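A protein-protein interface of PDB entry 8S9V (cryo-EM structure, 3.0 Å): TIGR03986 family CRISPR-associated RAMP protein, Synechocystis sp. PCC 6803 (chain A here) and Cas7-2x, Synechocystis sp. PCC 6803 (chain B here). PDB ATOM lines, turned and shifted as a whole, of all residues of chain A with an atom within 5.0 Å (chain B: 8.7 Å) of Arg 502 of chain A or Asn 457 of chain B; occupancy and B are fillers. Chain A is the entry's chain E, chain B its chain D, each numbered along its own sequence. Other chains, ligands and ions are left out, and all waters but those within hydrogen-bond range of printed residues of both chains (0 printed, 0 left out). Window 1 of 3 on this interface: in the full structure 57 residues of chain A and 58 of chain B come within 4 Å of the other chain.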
ATOM      1  N   LYS A 198       7.164 -24.268   6.172  1.00  0.00           N
ATOM      2  CA  LYS A 198       6.382 -25.489   6.295  1.00  0.00           C
ATOM      3  C   LYS A 198       7.255 -26.701   6.552  1.00  0.00           C
ATOM      4  O   LYS A 198       6.943 -27.523   7.412  1.00  0.00           O
ATOM      5  CB  LYS A 198       5.546 -25.697   5.046  1.00  0.00           C
ATOM      6  CG  LYS A 198       4.510 -26.749   5.185  1.00  0.00           C
ATOM      7  CD  LYS A 198       3.761 -26.901   3.905  1.00  0.00           C
ATOM      8  CE  LYS A 198       2.675 -27.906   4.055  1.00  0.00           C
ATOM      9  NZ  LYS A 198       2.064 -28.194   2.775  1.00  0.00           N
ATOM     10  N   LYS A 498      -4.958 -34.008   1.219  1.00  0.00           N
ATOM     11  CA  LYS A 498      -4.593 -32.613   1.377  1.00  0.00           C
ATOM     12  C   LYS A 498      -4.372 -32.266   2.829  1.00  0.00           C
ATOM     13  O   LYS A 498      -5.253 -32.444   3.655  1.00  0.00           O
ATOM     14  CB  LYS A 498      -5.669 -31.722   0.797  1.00  0.00           C
ATOM     15  CG  LYS A 498      -5.293 -30.287   0.806  1.00  0.00           C
ATOM     16  CD  LYS A 498      -6.338 -29.437   0.218  1.00  0.00           C
ATOM     17  CE  LYS A 498      -5.843 -28.054   0.201  1.00  0.00           C
ATOM     18  NZ  LYS A 498      -6.869 -27.117  -0.257  1.00  0.00           N
ATOM     19  N   GLY A 499      -3.247 -31.651   3.119  1.00  0.00           N
ATOM     20  CA  GLY A 499      -2.943 -31.299   4.485  1.00  0.00           C
ATOM     21  C   GLY A 499      -3.952 -30.355   5.098  1.00  0.00           C
ATOM     22  O   GLY A 499      -4.498 -29.476   4.449  1.00  0.00           O
ATOM     23  N   GLN A 500      -4.169 -30.541   6.382  1.00  0.00           N
ATOM     24  CA  GLN A 500      -4.971 -29.693   7.241  1.00  0.00           C
ATOM     25  C   GLN A 500      -4.248 -28.461   7.772  1.00  0.00           C
ATOM     26  O   GLN A 500      -4.844 -27.727   8.550  1.00  0.00           O
ATOM     27  CB  GLN A 500      -5.488 -30.559   8.376  1.00  0.00           C
ATOM     28  CG  GLN A 500      -6.578 -31.460   7.889  1.00  0.00           C
ATOM     29  CD  GLN A 500      -6.911 -32.550   8.826  1.00  0.00           C
ATOM     30  OE1 GLN A 500      -6.851 -33.708   8.466  1.00  0.00           O
ATOM     31  NE2 GLN A 500      -7.167 -32.209  10.055  1.00  0.00           N
ATOM     32  N   LEU A 501      -2.981 -28.230   7.443  1.00  0.00           N
ATOM     33  CA  LEU A 501      -2.256 -27.060   7.926  1.00  0.00           C
ATOM     34  C   LEU A 501      -1.698 -26.278   6.751  1.00  0.00           C
ATOM     35  O   LEU A 501      -0.898 -26.808   5.980  1.00  0.00           O
ATOM     36  CB  LEU A 501      -1.149 -27.487   8.877  1.00  0.00           C
ATOM     37  CG  LEU A 501      -0.387 -26.432   9.653  1.00  0.00           C
ATOM     38  CD1 LEU A 501       0.166 -27.091  10.864  1.00  0.00           C
ATOM     39  CD2 LEU A 501       0.734 -25.912   8.831  1.00  0.00           C
ATOM     40  N   ARG A 502      -2.094 -25.010   6.647  1.00  0.00           N
ATOM     41  CA  ARG A 502      -1.745 -24.100   5.557  1.00  0.00           C
ATOM     42  C   ARG A 502      -1.032 -22.872   6.091  1.00  0.00           C
ATOM     43  O   ARG A 502      -1.543 -22.211   6.989  1.00  0.00           O
ATOM     44  CB  ARG A 502      -2.994 -23.693   4.804  1.00  0.00           C
ATOM     45  CG  ARG A 502      -2.868 -22.497   3.956  1.00  0.00           C
ATOM     46  CD  ARG A 502      -4.213 -22.213   3.392  1.00  0.00           C
ATOM     47  NE  ARG A 502      -4.389 -20.827   3.006  1.00  0.00           N
ATOM     48  CZ  ARG A 502      -5.505 -20.151   3.254  1.00  0.00           C
ATOM     49  NH1 ARG A 502      -5.647 -18.907   2.834  1.00  0.00           N
ATOM     50  NH2 ARG A 502      -6.502 -20.734   3.907  1.00  0.00           N
ATOM     51  N   ILE A 503       0.129 -22.561   5.526  1.00  0.00           N
ATOM     52  CA  ILE A 503       0.942 -21.410   5.909  1.00  0.00           C
ATOM     53  C   ILE A 503       0.845 -20.347   4.829  1.00  0.00           C
ATOM     54  O   ILE A 503       0.991 -20.651   3.642  1.00  0.00           O
ATOM     55  CB  ILE A 503       2.400 -21.826   6.136  1.00  0.00           C
ATOM     56  CG1 ILE A 503       2.457 -22.898   7.201  1.00  0.00           C
ATOM     57  CG2 ILE A 503       3.236 -20.654   6.524  1.00  0.00           C
ATOM     58  CD1 ILE A 503       3.797 -23.208   7.622  1.00  0.00           C
ATOM     59  N   HIS A 504       0.568 -19.112   5.226  1.00  0.00           N
ATOM     60  CA  HIS A 504       0.272 -18.077   4.251  1.00  0.00           C
ATOM     61  C   HIS A 504       0.565 -16.703   4.831  1.00  0.00           C
ATOM     62  O   HIS A 504       0.840 -16.552   6.018  1.00  0.00           O
ATOM     63  CB  HIS A 504      -1.173 -18.217   3.770  1.00  0.00           C
ATOM     64  CG  HIS A 504      -2.213 -17.898   4.803  1.00  0.00           C
ATOM     65  ND1 HIS A 504      -2.693 -16.628   5.021  1.00  0.00           N
ATOM     66  CD2 HIS A 504      -2.884 -18.697   5.657  1.00  0.00           C
ATOM     67  CE1 HIS A 504      -3.601 -16.658   5.974  1.00  0.00           C
ATOM     68  NE2 HIS A 504      -3.733 -17.904   6.379  1.00  0.00           N
ATOM     69  N   GLU A 634       0.834 -16.430   8.930  1.00  0.00           N
ATOM     70  CA  GLU A 634      -0.368 -17.019   9.494  1.00  0.00           C
ATOM     71  C   GLU A 634      -0.478 -18.487   9.130  1.00  0.00           C
ATOM     72  O   GLU A 634      -0.163 -18.879   8.010  1.00  0.00           O
ATOM     73  CB  GLU A 634      -1.565 -16.237   9.020  1.00  0.00           C
ATOM     74  CG  GLU A 634      -1.588 -14.886   9.677  1.00  0.00           C
ATOM     75  CD  GLU A 634      -2.613 -13.962   9.115  1.00  0.00           C
ATOM     76  OE1 GLU A 634      -3.775 -14.368   8.982  1.00  0.00           O
ATOM     77  OE2 GLU A 634      -2.255 -12.811   8.813  1.00  0.00           O
ATOM     78  N   ILE A 635      -0.961 -19.287  10.069  1.00  0.00           N
ATOM     79  CA  ILE A 635      -1.268 -20.691   9.843  1.00  0.00           C
ATOM     80  C   ILE A 635      -2.775 -20.867   9.912  1.00  0.00           C
ATOM     81  O   ILE A 635      -3.405 -20.488  10.899  1.00  0.00           O
ATOM     82  CB  ILE A 635      -0.564 -21.590  10.865  1.00  0.00           C
ATOM     83  CG1 ILE A 635       0.913 -21.316  10.889  1.00  0.00           C
ATOM     84  CG2 ILE A 635      -0.729 -23.007  10.527  1.00  0.00           C
ATOM     85  CD1 ILE A 635       1.593 -22.128  11.883  1.00  0.00           C
ATOM     86  N   ASP A 636      -3.350 -21.422   8.861  1.00  0.00           N
ATOM     87  CA  ASP A 636      -4.772 -21.695   8.769  1.00  0.00           C
ATOM     88  C   ASP A 636      -4.949 -23.203   8.874  1.00  0.00           C
ATOM     89  O   ASP A 636      -4.410 -23.937   8.052  1.00  0.00           O
ATOM     90  CB  ASP A 636      -5.266 -21.144   7.437  1.00  0.00           C
ATOM     91  CG  ASP A 636      -6.759 -21.175   7.271  1.00  0.00           C
ATOM     92  OD1 ASP A 636      -7.450 -20.324   7.860  1.00  0.00           O
ATOM     93  OD2 ASP A 636      -7.241 -22.007   6.482  1.00  0.00           O
ATOM     94  N   PHE B 114     -11.131 -35.729   0.899  1.00  0.00           N
ATOM     95  CA  PHE B 114      -9.678 -35.713   0.936  1.00  0.00           C
ATOM     96  C   PHE B 114      -9.086 -34.441   0.374  1.00  0.00           C
ATOM     97  O   PHE B 114      -7.907 -34.186   0.587  1.00  0.00           O
ATOM     98  CB  PHE B 114      -9.093 -36.889   0.176  1.00  0.00           C
ATOM     99  CG  PHE B 114      -9.512 -38.211   0.692  1.00  0.00           C
ATOM    100  CD1 PHE B 114      -9.101 -38.630   1.931  1.00  0.00           C
ATOM    101  CD2 PHE B 114     -10.291 -39.048  -0.059  1.00  0.00           C
ATOM    102  CE1 PHE B 114      -9.471 -39.833   2.405  1.00  0.00           C
ATOM    103  CE2 PHE B 114     -10.664 -40.250   0.418  1.00  0.00           C
ATOM    104  CZ  PHE B 114     -10.256 -40.645   1.647  1.00  0.00           C
ATOM    105  N   GLY B 115      -9.853 -33.654  -0.360  1.00  0.00           N
ATOM    106  CA  GLY B 115      -9.322 -32.445  -0.928  1.00  0.00           C
ATOM    107  C   GLY B 115      -8.417 -32.652  -2.109  1.00  0.00           C
ATOM    108  O   GLY B 115      -7.654 -31.751  -2.452  1.00  0.00           O
ATOM    109  N   LYS B 231      -1.980 -12.186  -2.577  1.00  0.00           N
ATOM    110  CA  LYS B 231      -1.135 -12.009  -1.410  1.00  0.00           C
ATOM    111  C   LYS B 231       0.018 -12.987  -1.366  1.00  0.00           C
ATOM    112  O   LYS B 231       1.098 -12.636  -0.889  1.00  0.00           O
ATOM    113  CB  LYS B 231      -1.974 -12.210  -0.156  1.00  0.00           C
ATOM    114  CG  LYS B 231      -1.316 -11.889   1.141  1.00  0.00           C
ATOM    115  CD  LYS B 231      -0.928 -10.468   1.304  1.00  0.00           C
ATOM    116  CE  LYS B 231      -0.513 -10.241   2.734  1.00  0.00           C
ATOM    117  NZ  LYS B 231      -0.210  -8.822   2.981  1.00  0.00           N
ATOM    118  N   ASP B 232      -0.183 -14.197  -1.846  1.00  0.00           N
ATOM    119  CA  ASP B 232       0.797 -15.173  -2.251  1.00  0.00           C
ATOM    120  C   ASP B 232       0.579 -15.512  -3.716  1.00  0.00           C
ATOM    121  O   ASP B 232      -0.552 -15.464  -4.189  1.00  0.00           O
ATOM    122  CB  ASP B 232       0.686 -16.449  -1.417  1.00  0.00           C
ATOM    123  CG  ASP B 232       1.122 -16.263   0.016  1.00  0.00           C
ATOM    124  OD1 ASP B 232       2.154 -15.612   0.259  1.00  0.00           O
ATOM    125  OD2 ASP B 232       0.443 -16.793   0.910  1.00  0.00           O
ATOM    126  N   ARG B 277     -19.251 -26.875   2.314  1.00  0.00           N
ATOM    127  CA  ARG B 277     -18.712 -27.063   3.650  1.00  0.00           C
ATOM    128  C   ARG B 277     -19.532 -26.324   4.686  1.00  0.00           C
ATOM    129  O   ARG B 277     -19.716 -26.807   5.804  1.00  0.00           O
ATOM    130  CB  ARG B 277     -17.272 -26.593   3.692  1.00  0.00           C
ATOM    131  CG  ARG B 277     -16.599 -26.867   4.984  1.00  0.00           C
ATOM    132  CD  ARG B 277     -15.166 -26.449   4.964  1.00  0.00           C
ATOM    133  NE  ARG B 277     -14.430 -27.217   3.987  1.00  0.00           N
ATOM    134  CZ  ARG B 277     -13.698 -26.659   3.043  1.00  0.00           C
ATOM    135  NH1 ARG B 277     -13.058 -27.390   2.152  1.00  0.00           N
ATOM    136  NH2 ARG B 277     -13.575 -25.352   3.022  1.00  0.00           N
ATOM    137  N   ASP B 444     -16.294 -15.299   3.398  1.00  0.00           N
ATOM    138  CA  ASP B 444     -15.072 -16.078   3.571  1.00  0.00           C
ATOM    139  C   ASP B 444     -14.034 -15.759   2.519  1.00  0.00           C
ATOM    140  O   ASP B 444     -12.847 -15.662   2.824  1.00  0.00           O
ATOM    141  CB  ASP B 444     -15.388 -17.560   3.478  1.00  0.00           C
ATOM    142  CG  ASP B 444     -15.944 -18.110   4.737  1.00  0.00           C
ATOM    143  OD1 ASP B 444     -16.113 -17.343   5.700  1.00  0.00           O
ATOM    144  OD2 ASP B 444     -16.199 -19.327   4.766  1.00  0.00           O
ATOM    145  N   LEU B 445     -14.461 -15.554   1.283  1.00  0.00           N
ATOM    146  CA  LEU B 445     -13.537 -15.139   0.245  1.00  0.00           C
ATOM    147  C   LEU B 445     -12.759 -13.910   0.656  1.00  0.00           C
ATOM    148  O   LEU B 445     -11.537 -13.863   0.497  1.00  0.00           O
ATOM    149  CB  LEU B 445     -14.309 -14.893  -1.038  1.00  0.00           C
ATOM    150  CG  LEU B 445     -13.552 -14.576  -2.302  1.00  0.00           C
ATOM    151  CD1 LEU B 445     -12.839 -15.786  -2.743  1.00  0.00           C
ATOM    152  CD2 LEU B 445     -14.529 -14.185  -3.348  1.00  0.00           C
ATOM    153  N   ASN B 447     -12.156 -12.964   3.672  1.00  0.00           N
ATOM    154  CA  ASN B 447     -11.396 -13.224   4.885  1.00  0.00           C
ATOM    155  C   ASN B 447     -10.264 -14.223   4.676  1.00  0.00           C
ATOM    156  O   ASN B 447      -9.845 -14.873   5.632  1.00  0.00           O
ATOM    157  CB  ASN B 447     -12.335 -13.724   5.973  1.00  0.00           C
ATOM    158  CG  ASN B 447     -13.018 -12.607   6.704  1.00  0.00           C
ATOM    159  OD1 ASN B 447     -12.455 -11.978   7.589  1.00  0.00           O
ATOM    160  ND2 ASN B 447     -14.241 -12.344   6.328  1.00  0.00           N
ATOM    161  N   LYS B 448      -9.784 -14.384   3.449  1.00  0.00           N
ATOM    162  CA  LYS B 448      -8.703 -15.304   3.095  1.00  0.00           C
ATOM    163  C   LYS B 448      -9.011 -16.756   3.399  1.00  0.00           C
ATOM    164  O   LYS B 448      -8.091 -17.565   3.500  1.00  0.00           O
ATOM    165  CB  LYS B 448      -7.364 -14.908   3.709  1.00  0.00           C
ATOM    166  CG  LYS B 448      -6.965 -13.495   3.382  1.00  0.00           C
ATOM    167  CD  LYS B 448      -5.580 -13.173   3.863  1.00  0.00           C
ATOM    168  CE  LYS B 448      -5.489 -13.243   5.349  1.00  0.00           C
ATOM    169  NZ  LYS B 448      -4.215 -12.661   5.810  1.00  0.00           N
ATOM    170  N   LYS B 449     -10.277 -17.106   3.605  1.00  0.00           N
ATOM    171  CA  LYS B 449     -10.658 -18.486   3.874  1.00  0.00           C
ATOM    172  C   LYS B 449     -10.798 -19.322   2.616  1.00  0.00           C
ATOM    173  O   LYS B 449     -10.914 -20.539   2.716  1.00  0.00           O
ATOM    174  CB  LYS B 449     -11.968 -18.532   4.639  1.00  0.00           C
ATOM    175  CG  LYS B 449     -11.865 -18.258   6.107  1.00  0.00           C
ATOM    176  CD  LYS B 449     -13.254 -18.122   6.679  1.00  0.00           C
ATOM    177  CE  LYS B 449     -13.279 -18.159   8.174  1.00  0.00           C
ATOM    178  NZ  LYS B 449     -13.246 -19.561   8.652  1.00  0.00           N
ATOM    179  N   ILE B 450     -10.808 -18.712   1.442  1.00  0.00           N
ATOM    180  CA  ILE B 450     -10.894 -19.461   0.195  1.00  0.00           C
ATOM    181  C   ILE B 450      -9.665 -19.143  -0.644  1.00  0.00           C
ATOM    182  O   ILE B 450      -9.632 -18.109  -1.320  1.00  0.00           O
ATOM    183  CB  ILE B 450     -12.189 -19.151  -0.567  1.00  0.00           C
ATOM    184  CG1 ILE B 450     -13.392 -19.302   0.340  1.00  0.00           C
ATOM    185  CG2 ILE B 450     -12.351 -20.049  -1.731  1.00  0.00           C
ATOM    186  CD1 ILE B 450     -14.679 -19.035  -0.339  1.00  0.00           C
ATOM    187  N   PRO B 451      -8.607 -19.939  -0.549  1.00  0.00           N
ATOM    188  CA  PRO B 451      -7.491 -19.803  -1.473  1.00  0.00           C
ATOM    189  C   PRO B 451      -7.819 -20.418  -2.824  1.00  0.00           C
ATOM    190  O   PRO B 451      -8.676 -21.286  -2.951  1.00  0.00           O
ATOM    191  CB  PRO B 451      -6.379 -20.566  -0.764  1.00  0.00           C
ATOM    192  CG  PRO B 451      -7.072 -21.596  -0.078  1.00  0.00           C
ATOM    193  CD  PRO B 451      -8.378 -21.053   0.374  1.00  0.00           C
ATOM    194  N   VAL B 452      -7.081 -19.971  -3.832  1.00  0.00           N
ATOM    195  CA  VAL B 452      -7.387 -20.246  -5.226  1.00  0.00           C
ATOM    196  C   VAL B 452      -6.150 -20.771  -5.929  1.00  0.00           C
ATOM    197  O   VAL B 452      -5.028 -20.358  -5.633  1.00  0.00           O
ATOM    198  CB  VAL B 452      -7.945 -18.990  -5.923  1.00  0.00           C
ATOM    199  CG1 VAL B 452      -7.069 -17.834  -5.676  1.00  0.00           C
ATOM    200  CG2 VAL B 452      -8.060 -19.211  -7.399  1.00  0.00           C
ATOM    201  N   GLY B 453      -6.361 -21.682  -6.860  1.00  0.00           N
ATOM    202  CA  GLY B 453      -5.317 -22.203  -7.719  1.00  0.00           C
ATOM    203  C   GLY B 453      -4.432 -23.289  -7.126  1.00  0.00           C
ATOM    204  O   GLY B 453      -4.780 -23.982  -6.169  1.00  0.00           O
ATOM    205  N   TYR B 454      -3.266 -23.438  -7.748  1.00  0.00           N
ATOM    206  CA  TYR B 454      -2.318 -24.489  -7.420  1.00  0.00           C
ATOM    207  C   TYR B 454      -1.602 -24.216  -6.113  1.00  0.00           C
ATOM    208  O   TYR B 454      -1.333 -23.076  -5.760  1.00  0.00           O
ATOM    209  CB  TYR B 454      -1.283 -24.593  -8.534  1.00  0.00           C
ATOM    210  CG  TYR B 454      -0.398 -25.794  -8.474  1.00  0.00           C
ATOM    211  CD1 TYR B 454      -0.894 -27.036  -8.785  1.00  0.00           C
ATOM    212  CD2 TYR B 454       0.927 -25.691  -8.122  1.00  0.00           C
ATOM    213  CE1 TYR B 454      -0.118 -28.132  -8.746  1.00  0.00           C
ATOM    214  CE2 TYR B 454       1.715 -26.788  -8.065  1.00  0.00           C
ATOM    215  CZ  TYR B 454       1.182 -28.012  -8.381  1.00  0.00           C
ATOM    216  OH  TYR B 454       1.949 -29.148  -8.344  1.00  0.00           O
ATOM    217  N   GLY B 455      -1.251 -25.282  -5.413  1.00  0.00           N
ATOM    218  CA  GLY B 455      -0.325 -25.149  -4.318  1.00  0.00           C
ATOM    219  C   GLY B 455      -0.822 -24.344  -3.160  1.00  0.00           C
ATOM    220  O   GLY B 455      -0.036 -23.665  -2.522  1.00  0.00           O
ATOM    221  N   THR B 456      -2.116 -24.368  -2.885  1.00  0.00           N
ATOM    222  CA  THR B 456      -2.662 -23.521  -1.836  1.00  0.00           C
ATOM    223  C   THR B 456      -2.048 -23.824  -0.476  1.00  0.00           C
ATOM    224  O   THR B 456      -1.875 -22.918   0.341  1.00  0.00           O
ATOM    225  CB  THR B 456      -4.170 -23.655  -1.795  1.00  0.00           C
ATOM    226  OG1 THR B 456      -4.511 -25.009  -1.537  1.00  0.00           O
ATOM    227  CG2 THR B 456      -4.729 -23.308  -3.104  1.00  0.00           C
ATOM    228  N   ASN B 457      -1.701 -25.073  -0.216  1.00  0.00           N
ATOM    229  CA  ASN B 457      -1.055 -25.453   1.028  1.00  0.00           C
ATOM    230  C   ASN B 457       0.458 -25.341   0.982  1.00  0.00           C
ATOM    231  O   ASN B 457       1.120 -25.670   1.962  1.00  0.00           O
ATOM    232  CB  ASN B 457      -1.446 -26.876   1.374  1.00  0.00           C
ATOM    233  CG  ASN B 457      -2.611 -26.941   2.288  1.00  0.00           C
ATOM    234  OD1 ASN B 457      -3.334 -25.980   2.449  1.00  0.00           O
ATOM    235  ND2 ASN B 457      -2.815 -28.081   2.893  1.00  0.00           N
ATOM    236  N   ARG B 458       1.012 -24.860  -0.118  1.00  0.00           N
ATOM    237  CA  ARG B 458       2.424 -24.940  -0.451  1.00  0.00           C
ATOM    238  C   ARG B 458       2.902 -23.610  -0.989  1.00  0.00           C
ATOM    239  O   ARG B 458       3.632 -23.539  -1.977  1.00  0.00           O
ATOM    240  CB  ARG B 458       2.714 -26.101  -1.400  1.00  0.00           C
ATOM    241  CG  ARG B 458       2.162 -27.407  -0.872  1.00  0.00           C
ATOM    242  CD  ARG B 458       2.633 -28.654  -1.592  1.00  0.00           C
ATOM    243  NE  ARG B 458       2.476 -28.668  -3.031  1.00  0.00           N
ATOM    244  CZ  ARG B 458       1.301 -28.794  -3.616  1.00  0.00           C
ATOM    245  NH1 ARG B 458       1.179 -28.765  -4.924  1.00  0.00           N
ATOM    246  NH2 ARG B 458       0.243 -28.959  -2.865  1.00  0.00           N
ATOM    247  N   GLY B 459       2.456 -22.536  -0.347  1.00  0.00           N
ATOM    248  CA  GLY B 459       2.961 -21.203  -0.584  1.00  0.00           C
ATOM    249  C   GLY B 459       2.325 -20.417  -1.696  1.00  0.00           C
ATOM    250  O   GLY B 459       2.953 -19.492  -2.211  1.00  0.00           O
ATOM    251  N   MET B 460       1.114 -20.758  -2.099  1.00  0.00           N
ATOM    252  CA  MET B 460       0.445 -20.043  -3.161  1.00  0.00           C
ATOM    253  C   MET B 460      -1.019 -19.869  -2.809  1.00  0.00           C
ATOM    254  O   MET B 460      -1.523 -20.455  -1.863  1.00  0.00           O
ATOM    255  CB  MET B 460       0.638 -20.764  -4.488  1.00  0.00           C
ATOM    256  CG  MET B 460       2.007 -20.528  -5.063  1.00  0.00           C
ATOM    257  SD  MET B 460       2.228 -21.111  -6.723  1.00  0.00           S
ATOM    258  CE  MET B 460       2.574 -22.803  -6.372  1.00  0.00           C
ATOM    259  N   GLY B 461      -1.694 -19.021  -3.558  1.00  0.00           N
ATOM    260  CA  GLY B 461      -3.130 -19.074  -3.636  1.00  0.00           C
ATOM    261  C   GLY B 461      -3.941 -18.200  -2.710  1.00  0.00           C
ATOM    262  O   GLY B 461      -5.165 -18.275  -2.764  1.00  0.00           O
ATOM    263  N   THR B 462      -3.341 -17.370  -1.878  1.00  0.00           N
ATOM    264  CA  THR B 462      -4.122 -16.597  -0.924  1.00  0.00           C
ATOM    265  C   THR B 462      -4.348 -15.206  -1.495  1.00  0.00           C
ATOM    266  O   THR B 462      -3.401 -14.560  -1.941  1.00  0.00           O
ATOM    267  CB  THR B 462      -3.418 -16.526   0.429  1.00  0.00           C
ATOM    268  OG1 THR B 462      -4.387 -16.553   1.472  1.00  0.00           O
ATOM    269  CG2 THR B 462      -2.701 -15.262   0.570  1.00  0.00           C
ATOM    270  N   ILE B 463      -5.596 -14.744  -1.481  1.00  0.00           N
ATOM    271  CA  ILE B 463      -5.949 -13.514  -2.172  1.00  0.00           C
ATOM    272  C   ILE B 463      -6.431 -12.497  -1.159  1.00  0.00           C
ATOM    273  O   ILE B 463      -7.058 -12.835  -0.155  1.00  0.00           O
ATOM    274  CB  ILE B 463      -7.013 -13.715  -3.271  1.00  0.00           C
ATOM    275  CG1 ILE B 463      -8.356 -14.073  -2.687  1.00  0.00           C
ATOM    276  CG2 ILE B 463      -6.633 -14.811  -4.200  1.00  0.00           C
ATOM    277  CD1 ILE B 463      -9.429 -14.117  -3.719  1.00  0.00           C
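Of the 11 printed residues of chain A, 7 touch a printed residue of chain B. Hydrophobic or aromatic side chains of chain A within 4 Å of the printed part of chain B: His 504. Hydrophobic or aromatic side chains of chain B within 4 Å of the printed part of chain A: Pro 451. Among the printed residues, Asp or Glu carboxylates within 4 Å of a Lys or Arg side-chain nitrogen of the other chain: Glu 634 of chain A with Lys 448 of chain B (3.6 Å).
Printed residues of chain B within 4 Å of Lys 198 of chain A: Asn 457 and Arg 458. Printed residues of chain B within 4 Å of Leu 501 of chain A: Asn 457 (3.9 Å). Of the printed residues of chain B, Arg 502 of chain A touches Lys 448, Pro 451, Thr 456, Asn 457 and Thr 462. No residue of chain B comes within 4 Å of Asp 636 of chain A. Of the printed residues of chain A, Gly 115 of chain B touches Lys 498. Printed residues of chain A within 4 Å of Thr 456 of chain B: Lys 498 and Arg 502. Of chain A, only Lys 198 (2.8 Å), Lys 498 (3.9 Å), Gly 499 (2.7 Å), Leu 501 (3.9 Å) and Arg 502 (3.3 Å) come within 4 Å of Asn 457 of chain B. Ile 463 of chain B touches none of the printed residues of chain A. The nearest residue of chain B that does not touch Arg 502 of chain A is Lys 449 of chain B (4.6 Å). The nearest printed residue of chain B that does not touch His 504 of chain A is Thr 456 of chain B (5.9 Å).
The backbone NH of Lys 231 of chain B sits at hydrogen-bond distance from the backbone carbonyl oxygen of Thr 462 of chain B (2.8 Å). N of Asp 232 of chain B is in hydrogen-bond range of O of Thr 462 of chain B. The guanidinium group (NH2) of Arg 502 of chain A lies within salt-bridge range of the side-chain carboxylate (OD2) of Asp 636 of chain A, 3.0 Å away. The backbone carbonyl oxygen of Glu 634 of chain A lies within hydrogen-bond range of the backbone NH of His 504 of chain A (2.9 Å).
NZ of Lys 198 of chain A touches CG of Arg 458 of chain B, at 3.7 Å. Gly 115 of chain B touches Lys 498 of chain A. Asn 457 of chain B touches Lys 498 of chain A. Leu 501 of chain A touches Asn 457 of chain B (O to ND2, 3.9 Å). CZ of Arg 502 of chain A touches CG of Pro 451 of chain B, at 3.96 Å. O of Thr 456 of chain B touches CG of Arg 502 of chain A (3.8 Å). Arg 502 of chain A touches Asn 457 of chain B (CB to OD1, 3.3 Å). His 504 of chain A touches Asp 232 of chain B (CB to OD2, 3.6 Å). Lys 448 of chain B touches His 504 of chain A. ND1 of His 504 of chain A touches OG1 of Thr 462 of chain B, at 3.9 Å.
The backbone carbonyl oxygen (O) of Phe 114 of chain B sits at hydrogen-bond distance from the backbone NH (N) of Lys 498 of chain A (3.0 Å). O of Lys 448 of chain B is in hydrogen-bond range of NH1 of Arg 502 of chain A, at 2.9 Å. OE2 of Glu 634 of chain A lies within salt-bridge range of NZ of Lys 448 of chain B (3.6 Å). The side-chain amino group of Lys 498 of chain A is in hydrogen-bond range of the side-chain hydroxyl of Thr 456 of chain B, 3.4 Å away. The side-chain amino group (NZ) of Lys 198 of chain A lies within hydrogen-bond range of the backbone carbonyl oxygen (O) of Asn 457 of chain B, 2.8 Å away. The side-chain amide nitrogen (ND2) of Asn 457 of chain B is in hydrogen-bond range of the backbone carbonyl oxygen (O) of Gly 499 of chain A, 2.7 Å away. The guanidinium group of Arg 502 of chain A is in hydrogen-bond range of the side-chain hydroxyl of Thr 462 of chain B, at 3.0 Å.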
